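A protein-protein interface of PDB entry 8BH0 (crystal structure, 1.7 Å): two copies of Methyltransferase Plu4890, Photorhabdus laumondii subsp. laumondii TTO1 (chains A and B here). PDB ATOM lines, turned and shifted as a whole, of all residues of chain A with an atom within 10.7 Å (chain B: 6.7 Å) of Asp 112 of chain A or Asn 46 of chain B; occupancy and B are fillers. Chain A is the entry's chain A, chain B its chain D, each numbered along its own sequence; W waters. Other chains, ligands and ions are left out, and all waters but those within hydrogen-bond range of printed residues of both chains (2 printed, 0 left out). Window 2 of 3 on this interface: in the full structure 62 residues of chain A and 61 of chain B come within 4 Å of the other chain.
The backbone carbonyl oxygen (O) of Ser 108 of chain A lies within hydrogen-bond range of the guanidinium group (NH1) of Arg 49 of chain B (2.8 Å).
O of Leu 109 of chain A lies within hydrogen-bond range of N of Asn 46 of chain B (2.7 Å).
The side-chain amide nitrogen of Asn 46 of chain B lies within hydrogen-bond range of the side-chain carboxylate of Asp 112 of chain A (3.2 Å).
The side-chain carboxylate of Asp 274 of chain A is in salt-bridge range of the guanidinium group of Arg 49 of chain B, 2.8 Å away.
O of Tyr 105 of chain A sits at hydrogen-bond distance from OG of Ser 108 of chain A (2.6 Å).
The side-chain hydroxyl (OG) of Ser 40 of chain B is in hydrogen-bond range of the backbone carbonyl oxygen (O) of Val 45 of chain B.
The backbone NH (N) of Val 45 of chain B sits at hydrogen-bond distance from the side-chain hydroxyl (OG) of Ser 43 of chain B (3.2 Å).
The side-chain amide oxygen (OD1) of Asn 46 of chain B lies within hydrogen-bond range of the backbone NH (N) of Ala 48 of chain B, at 3.3 Å.
The side-chain amide oxygen (OD1) of Asn 46 of chain B sits at hydrogen-bond distance from the backbone NH (N) of Arg 49 of chain B, at 2.9 Å.
Among the printed residues, pairs that only touch across the chains: Leu 109 of chain A with Val 45 of chain B (3.4 Å), Leu 278 of chain A with Arg 49 of chain B (3.5 Å), Phe 110 of chain A with Ser 43 of chain B (3.6 Å), Leu 109 of chain A with Arg 49 of chain B (3.7 Å), Phe 110 of chain A with Val 45 of chain B (3.8 Å) and Phe 110 of chain A with Gly 44 of chain B (3.9 Å).
Printed residues of chain B within 4 Å of Ser 108 of chain A: Arg 49.
Of the printed residues of chain B, Leu 109 of chain A touches Val 45, Asn 46 and Arg 49.
Of chain B, only Asn 46 comes within 4 Å of Asp 112 of chain A.
Printed residues of chain B within 4 Å of Asp 274 of chain A: Arg 49 (2.8 Å).
Of the printed residues of chain B, Leu 278 of chain A touches Arg 49.
Ser 40 of chain B touches none of the printed residues of chain A.
Of the printed residues of chain A, Ser 43 of chain B touches Phe 110 (3.6 Å).
Val 45 of chain B touches just these residues of chain A: Leu 109 (3.4 Å) and Phe 110 (3.8 Å).
Of chain A, only Leu 109 and Asp 112 come within 4 Å of Asn 46 of chain B.
No residue of chain A comes within 4 Å of Ala 48 of chain B.
The nearest printed residue of chain B that does not touch Asp 112 of chain A is Arg 49 of chain B (5.4 Å).
The nearest printed residue of chain B that does not touch Asp 274 of chain A is Phe 50 of chain B (6.3 Å).
Of the 21 printed residues of chain A, 6 touch a printed residue of chain B.
Printed residues of chain A that touch a printed residue of chain B: Ser 108, Leu 109, Phe 110, Asp 112, Asp 274 and Leu 278.
Hydrophobic or aromatic side chains of chain A within 4 Å of the printed part of chain B: Leu 109, Phe 110 and Leu 278.
Printed residues of chain B that touch a printed residue of chain A: Ser 43, Gly 44, Val 45, Asn 46 and Arg 49.
No position is printed for both chains.
Of the 10 pairs that touch across the chains among the printed residues, none has its exchanged pair printed and touching as well.
Water W1 lies within hydrogen-bond range of OH of Tyr 105 of chain A (2.6 Å), OD2 of Asp 274 of chain A (2.7 Å) and O of Arg 49 of chain B (2.8 Å).
Water W2 lies within hydrogen-bond range of N of Ala 117 of chain A (2.8 Å), O of Asp 274 of chain A (2.8 Å) and NH2 of Arg 49 of chain B (3.2 Å).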
ATOM      1  N   MET A 104      21.724  -1.479  10.888  1.00  0.00           N
ATOM      2  CA  MET A 104      20.949  -0.479  11.675  1.00  0.00           C
ATOM      3  C   MET A 104      21.382   0.950  11.320  1.00  0.00           C
ATOM      4  O   MET A 104      20.716   1.892  11.791  1.00  0.00           O
ATOM      5  CB  MET A 104      21.141  -0.699  13.179  1.00  0.00           C
ATOM      6  CG  MET A 104      20.394  -1.898  13.719  1.00  0.00           C
ATOM      7  SD  MET A 104      18.598  -1.691  13.600  1.00  0.00           S
ATOM      8  CE  MET A 104      18.052  -2.879  14.826  1.00  0.00           C
ATOM      9  N   TYR A 105      22.439   1.120  10.519  1.00  0.00           N
ATOM     10  CA  TYR A 105      23.054   2.443  10.225  1.00  0.00           C
ATOM     11  C   TYR A 105      22.011   3.372   9.586  1.00  0.00           C
ATOM     12  O   TYR A 105      21.862   4.513  10.058  1.00  0.00           O
ATOM     13  CB  TYR A 105      24.294   2.286   9.342  1.00  0.00           C
ATOM     14  CG  TYR A 105      24.928   3.582   8.900  1.00  0.00           C
ATOM     15  CD1 TYR A 105      25.022   4.670   9.754  1.00  0.00           C
ATOM     16  CD2 TYR A 105      25.453   3.716   7.626  1.00  0.00           C
ATOM     17  CE1 TYR A 105      25.607   5.860   9.347  1.00  0.00           C
ATOM     18  CE2 TYR A 105      26.042   4.897   7.204  1.00  0.00           C
ATOM     19  CZ  TYR A 105      26.121   5.973   8.068  1.00  0.00           C
ATOM     20  OH  TYR A 105      26.702   7.139   7.657  1.00  0.00           O
ATOM     21  N   GLY A 106      21.316   2.895   8.550  1.00  0.00           N
ATOM     22  CA  GLY A 106      20.246   3.642   7.860  1.00  0.00           C
ATOM     23  C   GLY A 106      19.188   4.125   8.838  1.00  0.00           C
ATOM     24  O   GLY A 106      18.914   5.337   8.862  1.00  0.00           O
ATOM     25  N   LYS A 107      18.635   3.210   9.636  1.00  0.00           N
ATOM     26  CA  LYS A 107      17.589   3.497  10.654  1.00  0.00           C
ATOM     27  C   LYS A 107      18.108   4.503  11.691  1.00  0.00           C
ATOM     28  O   LYS A 107      17.312   5.356  12.122  1.00  0.00           O
ATOM     29  CB  LYS A 107      17.145   2.207  11.348  1.00  0.00           C
ATOM     30  CG  LYS A 107      16.176   1.343  10.550  1.00  0.00           C
ATOM     31  CD  LYS A 107      15.435   0.321  11.388  1.00  0.00           C
ATOM     32  CE  LYS A 107      14.781   0.915  12.621  1.00  0.00           C
ATOM     33  NZ  LYS A 107      13.686   0.057  13.133  1.00  0.00           N
ATOM     34  N   SER A 108      19.387   4.405  12.075  1.00  0.00           N
ATOM     35  CA  SER A 108      20.028   5.248  13.121  1.00  0.00           C
ATOM     36  C   SER A 108      20.046   6.724  12.700  1.00  0.00           C
ATOM     37  O   SER A 108      20.077   7.586  13.596  1.00  0.00           O
ATOM     38  CB  SER A 108      21.420   4.768  13.445  1.00  0.00           C
ATOM     39  OG  SER A 108      22.351   5.216  12.472  1.00  0.00           O
ATOM     40  N   LEU A 109      20.039   7.011  11.395  1.00  0.00           N
ATOM     41  CA  LEU A 109      20.105   8.402  10.866  1.00  0.00           C
ATOM     42  C   LEU A 109      18.783   9.143  11.117  1.00  0.00           C
ATOM     43  O   LEU A 109      18.782  10.380  10.962  1.00  0.00           O
ATOM     44  CB  LEU A 109      20.439   8.365   9.372  1.00  0.00           C
ATOM     45  CG  LEU A 109      21.859   7.922   9.022  1.00  0.00           C
ATOM     46  CD1 LEU A 109      21.987   7.659   7.530  1.00  0.00           C
ATOM     47  CD2 LEU A 109      22.881   8.955   9.472  1.00  0.00           C
ATOM     48  N   PHE A 110      17.711   8.431  11.490  1.00  0.00           N
ATOM     49  CA  PHE A 110      16.343   8.986  11.688  1.00  0.00           C
ATOM     50  C   PHE A 110      15.974   9.052  13.177  1.00  0.00           C
ATOM     51  O   PHE A 110      14.805   9.373  13.474  1.00  0.00           O
ATOM     52  CB  PHE A 110      15.321   8.150  10.914  1.00  0.00           C
ATOM     53  CG  PHE A 110      15.426   8.276   9.417  1.00  0.00           C
ATOM     54  CD1 PHE A 110      14.756   9.287   8.744  1.00  0.00           C
ATOM     55  CD2 PHE A 110      16.204   7.395   8.682  1.00  0.00           C
ATOM     56  CE1 PHE A 110      14.859   9.410   7.367  1.00  0.00           C
ATOM     57  CE2 PHE A 110      16.305   7.519   7.305  1.00  0.00           C
ATOM     58  CZ  PHE A 110      15.634   8.526   6.651  1.00  0.00           C
ATOM     59  N   GLU A 111      16.924   8.784  14.081  1.00  0.00           N
ATOM     60  CA  GLU A 111      16.683   8.755  15.550  1.00  0.00           C
ATOM     61  C   GLU A 111      17.688   9.668  16.261  1.00  0.00           C
ATOM     62  O   GLU A 111      18.832   9.785  15.775  1.00  0.00           O
ATOM     63  CB  GLU A 111      16.768   7.319  16.074  1.00  0.00           C
ATOM     64  CG  GLU A 111      15.887   6.344  15.312  1.00  0.00           C
ATOM     65  CD  GLU A 111      15.597   5.031  16.019  1.00  0.00           C
ATOM     66  OE1 GLU A 111      15.075   4.111  15.356  1.00  0.00           O
ATOM     67  OE2 GLU A 111      15.885   4.928  17.229  1.00  0.00           O
ATOM     68  N   ASP A 112      17.260  10.288  17.367  1.00  0.00           N
ATOM     69  CA  ASP A 112      18.090  11.166  18.236  1.00  0.00           C
ATOM     70  C   ASP A 112      17.897  10.751  19.702  1.00  0.00           C
ATOM     71  O   ASP A 112      17.814  11.648  20.567  1.00  0.00           O
ATOM     72  CB  ASP A 112      17.756  12.643  18.006  1.00  0.00           C
ATOM     73  CG  ASP A 112      18.043  13.127  16.595  1.00  0.00           C
ATOM     74  OD1 ASP A 112      19.128  12.800  16.071  1.00  0.00           O
ATOM     75  OD2 ASP A 112      17.179  13.825  16.027  1.00  0.00           O
ATOM     76  N   ASP A 113      17.837   9.439  19.962  1.00  0.00           N
ATOM     77  CA  ASP A 113      17.834   8.848  21.330  1.00  0.00           C
ATOM     78  C   ASP A 113      19.258   8.895  21.892  1.00  0.00           C
ATOM     79  O   ASP A 113      19.413   8.760  23.122  1.00  0.00           O
ATOM     80  CB  ASP A 113      17.328   7.403  21.331  1.00  0.00           C
ATOM     81  CG  ASP A 113      15.963   7.213  20.692  1.00  0.00           C
ATOM     82  OD1 ASP A 113      15.177   8.181  20.686  1.00  0.00           O
ATOM     83  OD2 ASP A 113      15.698   6.096  20.204  1.00  0.00           O
ATOM     84  N   GLY A 114      20.253   9.072  21.016  1.00  0.00           N
ATOM     85  CA  GLY A 114      21.687   9.017  21.349  1.00  0.00           C
ATOM     86  C   GLY A 114      22.202   7.592  21.330  1.00  0.00           C
ATOM     87  O   GLY A 114      23.287   7.350  21.896  1.00  0.00           O
ATOM     88  N   LYS A 115      21.450   6.685  20.697  1.00  0.00           N
ATOM     89  CA  LYS A 115      21.837   5.267  20.499  1.00  0.00           C
ATOM     90  C   LYS A 115      22.525   5.138  19.140  1.00  0.00           C
ATOM     91  O   LYS A 115      21.890   5.460  18.111  1.00  0.00           O
ATOM     92  CB  LYS A 115      20.616   4.348  20.603  1.00  0.00           C
ATOM     93  CG  LYS A 115      19.897   4.400  21.943  1.00  0.00           C
ATOM     94  CD  LYS A 115      18.788   3.383  22.084  1.00  0.00           C
ATOM     95  CE  LYS A 115      17.970   3.587  23.342  1.00  0.00           C
ATOM     96  NZ  LYS A 115      17.459   2.304  23.877  1.00  0.00           N
ATOM     97  N   SER A 116      23.785   4.704  19.150  1.00  0.00           N
ATOM     98  CA  SER A 116      24.559   4.317  17.944  1.00  0.00           C
ATOM     99  C   SER A 116      23.834   3.175  17.225  1.00  0.00           C
ATOM    100  O   SER A 116      23.029   2.473  17.878  1.00  0.00           O
ATOM    101  CB  SER A 116      25.959   3.915  18.319  1.00  0.00           C
ATOM    102  OG  SER A 116      25.939   2.741  19.120  1.00  0.00           O
ATOM    103  N   ALA A 117      24.121   2.984  15.937  1.00  0.00           N
ATOM    104  CA  ALA A 117      23.668   1.813  15.153  1.00  0.00           C
ATOM    105  C   ALA A 117      24.065   0.529  15.893  1.00  0.00           C
ATOM    106  O   ALA A 117      23.252  -0.412  15.928  1.00  0.00           O
ATOM    107  CB  ALA A 117      24.242   1.863  13.759  1.00  0.00           C
ATOM    108  N   GLU A 119      24.450   0.146  19.236  1.00  0.00           N
ATOM    109  CA  GLU A 119      23.559   0.029  20.421  1.00  0.00           C
ATOM    110  C   GLU A 119      22.154  -0.399  19.975  1.00  0.00           C
ATOM    111  O   GLU A 119      21.516  -1.171  20.717  1.00  0.00           O
ATOM    112  CB  GLU A 119      23.492   1.332  21.216  1.00  0.00           C
ATOM    113  CG  GLU A 119      22.584   1.221  22.429  1.00  0.00           C
ATOM    114  CD  GLU A 119      22.704   2.326  23.462  1.00  0.00           C
ATOM    115  OE1 GLU A 119      23.555   3.218  23.286  1.00  0.00           O
ATOM    116  OE2 GLU A 119      21.938   2.285  24.446  1.00  0.00           O
ATOM    117  N   MET A 120      21.686   0.084  18.822  1.00  0.00           N
ATOM    118  CA  MET A 120      20.354  -0.285  18.268  1.00  0.00           C
ATOM    119  C   MET A 120      20.327  -1.785  17.948  1.00  0.00           C
ATOM    120  O   MET A 120      19.266  -2.413  18.155  1.00  0.00           O
ATOM    121  CB  MET A 120      20.034   0.523  17.007  1.00  0.00           C
ATOM    122  CG  MET A 120      19.711   1.969  17.304  1.00  0.00           C
ATOM    123  SD  MET A 120      19.576   2.962  15.806  1.00  0.00           S
ATOM    124  CE  MET A 120      18.082   2.285  15.086  1.00  0.00           C
ATOM    125  N   ILE A 271      32.772   7.167   9.131  1.00  0.00           N
ATOM    126  CA  ILE A 271      31.434   6.507   9.087  1.00  0.00           C
ATOM    127  C   ILE A 271      31.434   5.335  10.076  1.00  0.00           C
ATOM    128  O   ILE A 271      30.426   5.184  10.787  1.00  0.00           O
ATOM    129  CB  ILE A 271      31.050   6.084   7.654  1.00  0.00           C
ATOM    130  CG1 ILE A 271      31.151   7.249   6.663  1.00  0.00           C
ATOM    131  CG2 ILE A 271      29.662   5.462   7.644  1.00  0.00           C
ATOM    132  CD1 ILE A 271      30.410   8.504   7.091  1.00  0.00           C
ATOM    133  N   ASP A 274      30.874   6.667  13.478  1.00  0.00           N
ATOM    134  CA  ASP A 274      29.439   7.029  13.627  1.00  0.00           C
ATOM    135  C   ASP A 274      28.652   5.774  14.028  1.00  0.00           C
ATOM    136  O   ASP A 274      27.901   5.831  15.021  1.00  0.00           O
ATOM    137  CB  ASP A 274      28.874   7.653  12.349  1.00  0.00           C
ATOM    138  CG  ASP A 274      27.487   8.240  12.537  1.00  0.00           C
ATOM    139  OD1 ASP A 274      27.266   8.905  13.568  1.00  0.00           O
ATOM    140  OD2 ASP A 274      26.632   8.015  11.661  1.00  0.00           O
ATOM    141  N   LEU A 278      28.668   6.728  17.635  1.00  0.00           N
ATOM    142  CA  LEU A 278      28.268   8.133  17.337  1.00  0.00           C
ATOM    143  C   LEU A 278      29.489   9.027  17.587  1.00  0.00           C
ATOM    144  O   LEU A 278      29.332  10.131  18.150  1.00  0.00           O
ATOM    145  CB  LEU A 278      27.075   8.551  18.205  1.00  0.00           C
ATOM    146  CG  LEU A 278      25.751   7.857  17.892  1.00  0.00           C
ATOM    147  CD1 LEU A 278      24.697   8.217  18.927  1.00  0.00           C
ATOM    148  CD2 LEU A 278      25.268   8.210  16.494  1.00  0.00           C
ATOM    149  N   GLY A 279      30.667   8.531  17.200  1.00  0.00           N
ATOM    150  CA  GLY A 279      31.930   9.287  17.196  1.00  0.00           C
ATOM    151  C   GLY A 279      32.157   9.926  15.841  1.00  0.00           C
ATOM    152  O   GLY A 279      31.216   9.945  15.023  1.00  0.00           O
ATOM    153  N   LYS A 280      33.362  10.437  15.606  1.00  0.00           N
ATOM    154  CA  LYS A 280      33.738  11.093  14.331  1.00  0.00           C
ATOM    155  C   LYS A 280      35.253  11.279  14.299  1.00  0.00           C
ATOM    156  O   LYS A 280      35.866  11.328  15.383  1.00  0.00           O
ATOM    157  CB  LYS A 280      33.037  12.448  14.193  1.00  0.00           C
ATOM    158  CG  LYS A 280      33.302  13.438  15.320  1.00  0.00           C
ATOM    159  CD  LYS A 280      32.922  14.863  14.977  1.00  0.00           C
ATOM    160  CE  LYS A 280      31.427  15.094  14.929  1.00  0.00           C
ATOM    161  NZ  LYS A 280      30.863  15.325  16.278  1.00  0.00           N
ATOM    162  N   ILE B  36      20.621  19.201   2.277  1.00  0.00           N
ATOM    163  CA  ILE B  36      20.443  18.206   3.379  1.00  0.00           C
ATOM    164  C   ILE B  36      19.640  18.859   4.513  1.00  0.00           C
ATOM    165  O   ILE B  36      18.870  18.138   5.170  1.00  0.00           O
ATOM    166  CB  ILE B  36      21.792  17.637   3.867  1.00  0.00           C
ATOM    167  CG1 ILE B  36      22.612  17.032   2.723  1.00  0.00           C
ATOM    168  CG2 ILE B  36      21.575  16.630   4.989  1.00  0.00           C
ATOM    169  CD1 ILE B  36      21.846  16.066   1.847  1.00  0.00           C
ATOM    170  N   SER B  40      16.370  17.113   5.831  1.00  0.00           N
ATOM    171  CA  SER B  40      16.250  16.850   7.290  1.00  0.00           C
ATOM    172  C   SER B  40      14.868  17.290   7.788  1.00  0.00           C
ATOM    173  O   SER B  40      14.234  16.510   8.523  1.00  0.00           O
ATOM    174  CB  SER B  40      17.358  17.522   8.061  1.00  0.00           C
ATOM    175  OG  SER B  40      17.204  17.310   9.456  1.00  0.00           O
ATOM    176  N   SER B  43      12.088  14.807   5.954  1.00  0.00           N
ATOM    177  CA  SER B  43      12.297  13.340   6.114  1.00  0.00           C
ATOM    178  C   SER B  43      12.603  12.976   7.575  1.00  0.00           C
ATOM    179  O   SER B  43      12.293  11.832   7.972  1.00  0.00           O
ATOM    180  CB  SER B  43      13.386  12.843   5.195  1.00  0.00           C
ATOM    181  OG  SER B  43      14.671  13.164   5.705  1.00  0.00           O
ATOM    182  N   GLY B  44      13.217  13.891   8.332  1.00  0.00           N
ATOM    183  CA  GLY B  44      13.624  13.669   9.733  1.00  0.00           C
ATOM    184  C   GLY B  44      15.019  13.073   9.843  1.00  0.00           C
ATOM    185  O   GLY B  44      15.430  12.758  10.978  1.00  0.00           O
ATOM    186  N   VAL B  45      15.735  12.921   8.722  1.00  0.00           N
ATOM    187  CA  VAL B  45      17.133  12.393   8.705  1.00  0.00           C
ATOM    188  C   VAL B  45      18.031  13.410   9.421  1.00  0.00           C
ATOM    189  O   VAL B  45      17.794  14.624   9.266  1.00  0.00           O
ATOM    190  CB  VAL B  45      17.630  12.089   7.277  1.00  0.00           C
ATOM    191  CG1 VAL B  45      17.936  13.351   6.483  1.00  0.00           C
ATOM    192  CG2 VAL B  45      18.836  11.163   7.293  1.00  0.00           C
ATOM    193  N   ASN B  46      19.005  12.923  10.194  1.00  0.00           N
ATOM    194  CA  ASN B  46      19.965  13.763  10.958  1.00  0.00           C
ATOM    195  C   ASN B  46      20.847  14.525   9.962  1.00  0.00           C
ATOM    196  O   ASN B  46      21.529  13.858   9.158  1.00  0.00           O
ATOM    197  CB  ASN B  46      20.803  12.925  11.925  1.00  0.00           C
ATOM    198  CG  ASN B  46      21.687  13.764  12.823  1.00  0.00           C
ATOM    199  OD1 ASN B  46      22.757  14.210  12.414  1.00  0.00           O
ATOM    200  ND2 ASN B  46      21.249  13.981  14.052  1.00  0.00           N
ATOM    201  N   TYR B  47      20.834  15.862  10.013  1.00  0.00           N
ATOM    202  CA  TYR B  47      21.584  16.745   9.081  1.00  0.00           C
ATOM    203  C   TYR B  47      23.082  16.418   9.116  1.00  0.00           C
ATOM    204  O   TYR B  47      23.649  16.072   8.063  1.00  0.00           O
ATOM    205  CB  TYR B  47      21.397  18.229   9.405  1.00  0.00           C
ATOM    206  CG  TYR B  47      22.335  19.111   8.621  1.00  0.00           C
ATOM    207  CD1 TYR B  47      22.060  19.442   7.305  1.00  0.00           C
ATOM    208  CD2 TYR B  47      23.529  19.559   9.165  1.00  0.00           C
ATOM    209  CE1 TYR B  47      22.927  20.225   6.560  1.00  0.00           C
ATOM    210  CE2 TYR B  47      24.408  20.341   8.434  1.00  0.00           C
ATOM    211  CZ  TYR B  47      24.105  20.676   7.125  1.00  0.00           C
ATOM    212  OH  TYR B  47      24.959  21.444   6.389  1.00  0.00           O
ATOM    213  N   ALA B  48      23.711  16.563  10.286  1.00  0.00           N
ATOM    214  CA  ALA B  48      25.177  16.450  10.476  1.00  0.00           C
ATOM    215  C   ALA B  48      25.655  15.058  10.044  1.00  0.00           C
ATOM    216  O   ALA B  48      26.646  14.969   9.292  1.00  0.00           O
ATOM    217  CB  ALA B  48      25.536  16.738  11.913  1.00  0.00           C
ATOM    218  N   ARG B  49      24.958  14.011  10.485  1.00  0.00           N
ATOM    219  CA  ARG B  49      25.378  12.600  10.290  1.00  0.00           C
ATOM    220  C   ARG B  49      25.121  12.177   8.837  1.00  0.00           C
ATOM    221  O   ARG B  49      25.987  11.482   8.272  1.00  0.00           O
ATOM    222  CB  ARG B  49      24.695  11.708  11.330  1.00  0.00           C
ATOM    223  CG  ARG B  49      25.191  11.969  12.748  1.00  0.00           C
ATOM    224  CD  ARG B  49      24.512  11.112  13.798  1.00  0.00           C
ATOM    225  NE  ARG B  49      24.637   9.705  13.449  1.00  0.00           N
ATOM    226  CZ  ARG B  49      23.640   8.827  13.376  1.00  0.00           C
ATOM    227  NH1 ARG B  49      22.399   9.177  13.673  1.00  0.00           N
ATOM    228  NH2 ARG B  49      23.899   7.580  13.019  1.00  0.00           N
ATOM    229  N   PHE B  50      24.005  12.588   8.226  1.00  0.00           N
ATOM    230  CA  PHE B  50      23.727  12.260   6.802  1.00  0.00           C
ATOM    231  C   PHE B  50      24.670  13.059   5.892  1.00  0.00           C
ATOM    232  O   PHE B  50      25.069  12.525   4.845  1.00  0.00           O
ATOM    233  CB  PHE B  50      22.266  12.485   6.408  1.00  0.00           C
ATOM    234  CG  PHE B  50      21.958  11.996   5.014  1.00  0.00           C
ATOM    235  CD1 PHE B  50      22.231  10.686   4.650  1.00  0.00           C
ATOM    236  CD2 PHE B  50      21.434  12.849   4.054  1.00  0.00           C
ATOM    237  CE1 PHE B  50      21.973  10.235   3.364  1.00  0.00           C
ATOM    238  CE2 PHE B  50      21.169  12.395   2.770  1.00  0.00           C
ATOM    239  CZ  PHE B  50      21.439  11.091   2.427  1.00  0.00           C
ATOM    240  N   SER B  51      25.015  14.294   6.265  1.00  0.00           N
ATOM    241  CA  SER B  51      25.999  15.129   5.522  1.00  0.00           C
ATOM    242  C   SER B  51      27.351  14.406   5.471  1.00  0.00           C
ATOM    243  O   SER B  51      27.978  14.409   4.399  1.00  0.00           O
ATOM    244  CB  SER B  51      26.124  16.508   6.115  1.00  0.00           C
ATOM    245  OG  SER B  51      24.934  17.249   5.901  1.00  0.00           O
HETATM  246  O   HOH W   1      27.101   9.150   9.266  1.00  0.00           O
HETATM  247  O   HOH W   2      25.218   5.193  14.663  1.00  0.00           O
